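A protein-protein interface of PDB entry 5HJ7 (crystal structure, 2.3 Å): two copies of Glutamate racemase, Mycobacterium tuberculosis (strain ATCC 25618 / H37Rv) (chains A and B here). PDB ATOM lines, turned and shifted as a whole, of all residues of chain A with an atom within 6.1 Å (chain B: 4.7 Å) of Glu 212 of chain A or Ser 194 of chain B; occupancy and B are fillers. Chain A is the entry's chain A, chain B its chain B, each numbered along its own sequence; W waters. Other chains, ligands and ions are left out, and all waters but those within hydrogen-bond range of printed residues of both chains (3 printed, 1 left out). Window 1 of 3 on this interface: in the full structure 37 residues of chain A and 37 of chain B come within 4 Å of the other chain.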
ATOM      1  N   THR A  21      39.667   7.463   3.856  1.00  0.00           N
ATOM      2  CA  THR A  21      38.325   7.980   3.580  1.00  0.00           C
ATOM      3  C   THR A  21      37.676   7.191   2.450  1.00  0.00           C
ATOM      4  O   THR A  21      36.472   6.908   2.494  1.00  0.00           O
ATOM      5  CB  THR A  21      38.345   9.473   3.220  1.00  0.00           C
ATOM      6  OG1 THR A  21      38.992   9.654   1.956  1.00  0.00           O
ATOM      7  CG2 THR A  21      39.061  10.300   4.287  1.00  0.00           C
ATOM      8  N   ALA A  25      34.576   4.340   2.870  1.00  0.00           N
ATOM      9  CA  ALA A  25      33.379   4.422   2.040  1.00  0.00           C
ATOM     10  C   ALA A  25      33.144   3.120   1.278  1.00  0.00           C
ATOM     11  O   ALA A  25      32.006   2.655   1.177  1.00  0.00           O
ATOM     12  CB  ALA A  25      33.486   5.607   1.075  1.00  0.00           C
ATOM     13  N   GLN A  29      29.852   0.394   1.828  1.00  0.00           N
ATOM     14  CA  GLN A  29      28.967  -0.121   0.789  1.00  0.00           C
ATOM     15  C   GLN A  29      29.095  -1.629   0.627  1.00  0.00           C
ATOM     16  O   GLN A  29      28.169  -2.276   0.139  1.00  0.00           O
ATOM     17  CB  GLN A  29      29.284   0.537  -0.551  1.00  0.00           C
ATOM     18  CG  GLN A  29      29.193   2.053  -0.566  1.00  0.00           C
ATOM     19  CD  GLN A  29      27.780   2.536  -0.341  1.00  0.00           C
ATOM     20  OE1 GLN A  29      26.846   2.063  -0.993  1.00  0.00           O
ATOM     21  NE2 GLN A  29      27.607   3.465   0.593  1.00  0.00           N
ATOM     22  N   SER A 209      32.374  14.405  -3.374  1.00  0.00           N
ATOM     23  CA  SER A 209      33.415  13.665  -2.669  1.00  0.00           C
ATOM     24  C   SER A 209      34.000  12.577  -3.566  1.00  0.00           C
ATOM     25  O   SER A 209      33.254  11.788  -4.151  1.00  0.00           O
ATOM     26  CB  SER A 209      32.841  13.034  -1.398  1.00  0.00           C
ATOM     27  OG  SER A 209      33.683  11.992  -0.945  1.00  0.00           O
ATOM     28  N   SER A 210      35.333  12.525  -3.671  1.00  0.00           N
ATOM     29  CA  SER A 210      35.951  11.423  -4.414  1.00  0.00           C
ATOM     30  C   SER A 210      35.643  10.086  -3.760  1.00  0.00           C
ATOM     31  O   SER A 210      35.346   9.100  -4.445  1.00  0.00           O
ATOM     32  CB  SER A 210      37.467  11.606  -4.505  1.00  0.00           C
ATOM     33  OG  SER A 210      37.785  12.897  -4.976  1.00  0.00           O
ATOM     34  N   ALA A 211      35.711  10.038  -2.432  1.00  0.00           N
ATOM     35  CA  ALA A 211      35.495   8.788  -1.708  1.00  0.00           C
ATOM     36  C   ALA A 211      34.107   8.226  -1.986  1.00  0.00           C
ATOM     37  O   ALA A 211      33.958   7.042  -2.298  1.00  0.00           O
ATOM     38  CB  ALA A 211      35.699   9.018  -0.208  1.00  0.00           C
ATOM     39  N   GLU A 212      33.084   9.079  -1.921  1.00  0.00           N
ATOM     40  CA  GLU A 212      31.704   8.628  -2.103  1.00  0.00           C
ATOM     41  C   GLU A 212      31.465   8.087  -3.514  1.00  0.00           C
ATOM     42  O   GLU A 212      30.935   6.977  -3.688  1.00  0.00           O
ATOM     43  CB  GLU A 212      30.746   9.784  -1.784  1.00  0.00           C
ATOM     44  CG  GLU A 212      29.254   9.487  -1.971  1.00  0.00           C
ATOM     45  CD  GLU A 212      28.763   8.328  -1.101  1.00  0.00           C
ATOM     46  OE1 GLU A 212      29.488   7.931  -0.153  1.00  0.00           O
ATOM     47  OE2 GLU A 212      27.647   7.815  -1.369  1.00  0.00           O
ATOM     48  N   GLU A 213      31.846   8.862  -4.537  1.00  0.00           N
ATOM     49  CA  GLU A 213      31.606   8.450  -5.916  1.00  0.00           C
ATOM     50  C   GLU A 213      32.404   7.195  -6.270  1.00  0.00           C
ATOM     51  O   GLU A 213      31.917   6.322  -7.001  1.00  0.00           O
ATOM     52  CB  GLU A 213      31.980   9.594  -6.860  1.00  0.00           C
ATOM     53  CG  GLU A 213      31.189  10.887  -6.701  1.00  0.00           C
ATOM     54  CD  GLU A 213      29.698  10.652  -6.444  1.00  0.00           C
ATOM     55  OE1 GLU A 213      29.126  11.272  -5.506  1.00  0.00           O
ATOM     56  OE2 GLU A 213      29.103   9.847  -7.193  1.00  0.00           O
ATOM     57  N   THR A 214      33.645   7.099  -5.780  1.00  0.00           N
ATOM     58  CA  THR A 214      34.460   5.926  -6.082  1.00  0.00           C
ATOM     59  C   THR A 214      33.882   4.667  -5.441  1.00  0.00           C
ATOM     60  O   THR A 214      33.841   3.604  -6.075  1.00  0.00           O
ATOM     61  CB  THR A 214      35.900   6.179  -5.640  1.00  0.00           C
ATOM     62  OG1 THR A 214      36.501   7.081  -6.571  1.00  0.00           O
ATOM     63  CG2 THR A 214      36.727   4.885  -5.589  1.00  0.00           C
ATOM     64  N   ALA A 215      33.391   4.769  -4.205  1.00  0.00           N
ATOM     65  CA  ALA A 215      32.813   3.595  -3.553  1.00  0.00           C
ATOM     66  C   ALA A 215      31.554   3.117  -4.276  1.00  0.00           C
ATOM     67  O   ALA A 215      31.358   1.906  -4.458  1.00  0.00           O
ATOM     68  CB  ALA A 215      32.516   3.899  -2.089  1.00  0.00           C
ATOM     69  N   LYS A 216      30.702   4.051  -4.725  1.00  0.00           N
ATOM     70  CA  LYS A 216      29.541   3.671  -5.530  1.00  0.00           C
ATOM     71  C   LYS A 216      29.956   3.025  -6.845  1.00  0.00           C
ATOM     72  O   LYS A 216      29.259   2.131  -7.343  1.00  0.00           O
ATOM     73  CB  LYS A 216      28.664   4.891  -5.800  1.00  0.00           C
ATOM     74  CG  LYS A 216      28.059   5.485  -4.531  1.00  0.00           C
ATOM     75  CD  LYS A 216      27.011   6.527  -4.852  1.00  0.00           C
ATOM     76  CE  LYS A 216      27.649   7.762  -5.477  1.00  0.00           C
ATOM     77  NZ  LYS A 216      26.657   8.842  -5.518  1.00  0.00           N
ATOM     78  N   GLU A 217      31.096   3.446  -7.401  1.00  0.00           N
ATOM     79  CA  GLU A 217      31.593   2.882  -8.652  1.00  0.00           C
ATOM     80  C   GLU A 217      32.142   1.477  -8.449  1.00  0.00           C
ATOM     81  O   GLU A 217      31.976   0.622  -9.323  1.00  0.00           O
ATOM     82  CB  GLU A 217      32.663   3.809  -9.247  1.00  0.00           C
ATOM     83  CG  GLU A 217      33.418   3.283 -10.465  1.00  0.00           C
ATOM     84  CD  GLU A 217      32.562   3.229 -11.720  1.00  0.00           C
ATOM     85  OE1 GLU A 217      31.408   3.696 -11.678  1.00  0.00           O
ATOM     86  OE2 GLU A 217      33.045   2.722 -12.758  1.00  0.00           O
ATOM     87  N   LEU B 185      17.972  10.761   0.582  1.00  0.00           N
ATOM     88  CA  LEU B 185      18.043   9.551   1.398  1.00  0.00           C
ATOM     89  C   LEU B 185      17.509   9.891   2.790  1.00  0.00           C
ATOM     90  O   LEU B 185      18.261  10.121   3.741  1.00  0.00           O
ATOM     91  CB  LEU B 185      19.472   9.022   1.437  1.00  0.00           C
ATOM     92  CG  LEU B 185      20.128   8.950   0.051  1.00  0.00           C
ATOM     93  CD1 LEU B 185      21.579   8.463   0.137  1.00  0.00           C
ATOM     94  CD2 LEU B 185      19.336   8.074  -0.907  1.00  0.00           C
ATOM     95  N   TYR B 190      20.174   4.780   5.033  1.00  0.00           N
ATOM     96  CA  TYR B 190      20.261   4.772   3.573  1.00  0.00           C
ATOM     97  C   TYR B 190      21.615   5.181   2.968  1.00  0.00           C
ATOM     98  O   TYR B 190      21.865   4.849   1.796  1.00  0.00           O
ATOM     99  CB  TYR B 190      19.145   5.649   2.991  1.00  0.00           C
ATOM    100  CG  TYR B 190      17.758   5.125   3.266  1.00  0.00           C
ATOM    101  CD1 TYR B 190      17.554   3.989   4.065  1.00  0.00           C
ATOM    102  CD2 TYR B 190      16.643   5.751   2.728  1.00  0.00           C
ATOM    103  CE1 TYR B 190      16.273   3.517   4.335  1.00  0.00           C
ATOM    104  CE2 TYR B 190      15.358   5.286   2.982  1.00  0.00           C
ATOM    105  CZ  TYR B 190      15.176   4.166   3.784  1.00  0.00           C
ATOM    106  OH  TYR B 190      13.890   3.713   4.049  1.00  0.00           O
ATOM    107  N   PRO B 191      22.511   5.890   3.679  1.00  0.00           N
ATOM    108  CA  PRO B 191      23.850   6.101   3.097  1.00  0.00           C
ATOM    109  C   PRO B 191      24.591   4.809   2.833  1.00  0.00           C
ATOM    110  O   PRO B 191      25.455   4.774   1.939  1.00  0.00           O
ATOM    111  CB  PRO B 191      24.566   6.961   4.151  1.00  0.00           C
ATOM    112  CG  PRO B 191      23.481   7.762   4.733  1.00  0.00           C
ATOM    113  CD  PRO B 191      22.303   6.792   4.829  1.00  0.00           C
ATOM    114  N   LEU B 192      24.275   3.741   3.570  1.00  0.00           N
ATOM    115  CA  LEU B 192      24.926   2.454   3.341  1.00  0.00           C
ATOM    116  C   LEU B 192      24.338   1.697   2.151  1.00  0.00           C
ATOM    117  O   LEU B 192      24.851   0.625   1.800  1.00  0.00           O
ATOM    118  CB  LEU B 192      24.864   1.597   4.601  1.00  0.00           C
ATOM    119  CG  LEU B 192      25.954   1.909   5.642  1.00  0.00           C
ATOM    120  CD1 LEU B 192      25.919   3.364   6.109  1.00  0.00           C
ATOM    121  CD2 LEU B 192      25.804   0.985   6.848  1.00  0.00           C
ATOM    122  N   LEU B 193      23.314   2.256   1.506  1.00  0.00           N
ATOM    123  CA  LEU B 193      22.756   1.761   0.257  1.00  0.00           C
ATOM    124  C   LEU B 193      23.023   2.678  -0.935  1.00  0.00           C
ATOM    125  O   LEU B 193      22.491   2.426  -2.019  1.00  0.00           O
ATOM    126  CB  LEU B 193      21.248   1.574   0.399  1.00  0.00           C
ATOM    127  CG  LEU B 193      20.772   0.381   1.216  1.00  0.00           C
ATOM    128  CD1 LEU B 193      19.272   0.495   1.472  1.00  0.00           C
ATOM    129  CD2 LEU B 193      21.112  -0.911   0.471  1.00  0.00           C
ATOM    130  N   SER B 194      23.805   3.746  -0.768  1.00  0.00           N
ATOM    131  CA  SER B 194      23.859   4.754  -1.832  1.00  0.00           C
ATOM    132  C   SER B 194      24.420   4.183  -3.131  1.00  0.00           C
ATOM    133  O   SER B 194      23.999   4.591  -4.215  1.00  0.00           O
ATOM    134  CB  SER B 194      24.666   5.972  -1.384  1.00  0.00           C
ATOM    135  OG  SER B 194      26.038   5.664  -1.194  1.00  0.00           O
ATOM    136  N   GLY B 195      25.344   3.227  -3.056  1.00  0.00           N
ATOM    137  CA  GLY B 195      25.811   2.587  -4.271  1.00  0.00           C
ATOM    138  C   GLY B 195      24.748   1.718  -4.913  1.00  0.00           C
ATOM    139  O   GLY B 195      24.633   1.663  -6.142  1.00  0.00           O
ATOM    140  N   LEU B 196      23.960   1.022  -4.092  1.00  0.00           N
ATOM    141  CA  LEU B 196      22.893   0.188  -4.633  1.00  0.00           C
ATOM    142  C   LEU B 196      21.807   1.050  -5.255  1.00  0.00           C
ATOM    143  O   LEU B 196      21.301   0.744  -6.345  1.00  0.00           O
ATOM    144  CB  LEU B 196      22.327  -0.697  -3.522  1.00  0.00           C
ATOM    145  CG  LEU B 196      21.370  -1.863  -3.784  1.00  0.00           C
ATOM    146  CD1 LEU B 196      19.970  -1.368  -3.997  1.00  0.00           C
ATOM    147  CD2 LEU B 196      21.819  -2.664  -4.976  1.00  0.00           C
ATOM    148  N   ILE B 197      21.461   2.151  -4.585  1.00  0.00           N
ATOM    149  CA  ILE B 197      20.422   3.033  -5.090  1.00  0.00           C
ATOM    150  C   ILE B 197      20.896   3.775  -6.328  1.00  0.00           C
ATOM    151  O   ILE B 197      20.143   3.919  -7.298  1.00  0.00           O
ATOM    152  CB  ILE B 197      19.974   3.998  -3.989  1.00  0.00           C
ATOM    153  CG1 ILE B 197      19.266   3.195  -2.893  1.00  0.00           C
ATOM    154  CG2 ILE B 197      19.090   5.092  -4.601  1.00  0.00           C
ATOM    155  CD1 ILE B 197      18.966   3.978  -1.651  1.00  0.00           C
ATOM    156  N   GLN B 198      22.139   4.275  -6.313  1.00  0.00           N
ATOM    157  CA  GLN B 198      22.673   4.932  -7.501  1.00  0.00           C
ATOM    158  C   GLN B 198      22.583   4.003  -8.701  1.00  0.00           C
ATOM    159  O   GLN B 198      22.199   4.425  -9.797  1.00  0.00           O
ATOM    160  CB  GLN B 198      24.122   5.366  -7.265  1.00  0.00           C
ATOM    161  CG  GLN B 198      24.688   6.316  -8.329  1.00  0.00           C
ATOM    162  CD  GLN B 198      24.093   7.704  -8.234  1.00  0.00           C
ATOM    163  OE1 GLN B 198      24.510   8.527  -7.415  1.00  0.00           O
ATOM    164  NE2 GLN B 198      23.104   7.972  -9.070  1.00  0.00           N
ATOM    165  N   LEU B 207      22.011  11.859  -5.375  1.00  0.00           N
ATOM    166  CA  LEU B 207      21.600  11.365  -4.071  1.00  0.00           C
ATOM    167  C   LEU B 207      22.012  12.358  -2.997  1.00  0.00           C
ATOM    168  O   LEU B 207      23.111  12.909  -3.039  1.00  0.00           O
ATOM    169  CB  LEU B 207      22.221   9.994  -3.794  1.00  0.00           C
ATOM    170  CG  LEU B 207      21.942   8.938  -4.882  1.00  0.00           C
ATOM    171  CD1 LEU B 207      22.449   7.533  -4.510  1.00  0.00           C
ATOM    172  CD2 LEU B 207      20.481   8.897  -5.215  1.00  0.00           C
HETATM  173  O   HOH W   1      27.208   7.202   1.604  1.00  0.00           O
HETATM  174  O   HOH W   2      26.680   2.117  -8.028  1.00  0.00           O
HETATM  175  O   HOH W   3      24.579  11.110  -6.567  1.00  0.00           O
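Water W2 lies within hydrogen-bond range of the backbone carbonyl oxygen (O) of Lys 216 of chain A (2.7 Å) and the backbone carbonyl oxygen (O) of Gly 195 of chain B (2.8 Å).
Water W3 lies within hydrogen-bond range of OE1 of Gln 198 of chain B (2.7 Å), N of Leu 207 of chain B (2.9 Å) and NZ of Lys 216 of chain A (3.2 Å).
Water W1 lies within hydrogen-bond range of the side-chain carboxylate (OE1) of Glu 212 of chain A (3.0 Å), the backbone carbonyl oxygen (O) of Pro 191 of chain B (3.0 Å) and the side-chain hydroxyl (OG) of Ser 194 of chain B (3.4 Å).
Glu 212 of chain A touches one residue of chain B.
Of chain A, only Gln 29, Glu 212 and Lys 216 come within 4 Å of Ser 194 of chain B.
Of the printed residues of chain B, Lys 216 of chain A touches Ser 194 (3.6 Å), Gly 195 (3.7 Å) and Gln 198 (2.9 Å).
Of the printed residues of chain A, Leu 193 of chain B touches Gln 29.
The nearest printed residue of chain A that does not touch Ser 194 of chain B is Ala 215 of chain A (6.8 Å).
No position is printed for both chains.
Of the 9 pairs that touch across the chains among the printed residues, none has its exchanged pair printed and touching as well.
Among the printed residues, merely in contact across the chains: Lys 216 of chain A with Ser 194 of chain B (3.6 Å), Lys 216 of chain A with Gly 195 of chain B (3.7 Å), Gln 29 of chain A with Leu 192 of chain B (3.7 Å) and Gln 29 of chain A with Leu 193 of chain B (3.9 Å).
The backbone NH (N) of Glu 212 of chain A is in hydrogen-bond range of the side-chain hydroxyl (OG) of Ser 209 of chain A, at 3.1 Å.
OE2 of Glu 213 of chain A is in salt-bridge range of NZ of Lys 216 of chain A (3.1 Å).
The backbone carbonyl oxygen of Pro 191 of chain B is in hydrogen-bond range of the side-chain hydroxyl of Ser 194 of chain B (3.3 Å).
Of the 11 printed residues of chain B, 6 touch a printed residue of chain A.
Among the printed residues, 9 pairs touch across the chains.
O of Pro 191 of chain B sits at hydrogen-bond distance from NE2 of Gln 29 of chain A, 2.9 Å away.
The side-chain amide nitrogen (NE2) of Gln 29 of chain A sits at hydrogen-bond distance from the side-chain hydroxyl (OG) of Ser 194 of chain B, at 3.2 Å.
The side-chain amide oxygen of Gln 29 of chain A is in hydrogen-bond range of the backbone NH of Gly 195 of chain B (2.8 Å).
OG of Ser 194 of chain B is in hydrogen-bond range of OE2 of Glu 212 of chain A.
The side-chain amino group (NZ) of Lys 216 of chain A is in hydrogen-bond range of the side-chain amide oxygen (OE1) of Gln 198 of chain B, 2.9 Å away.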
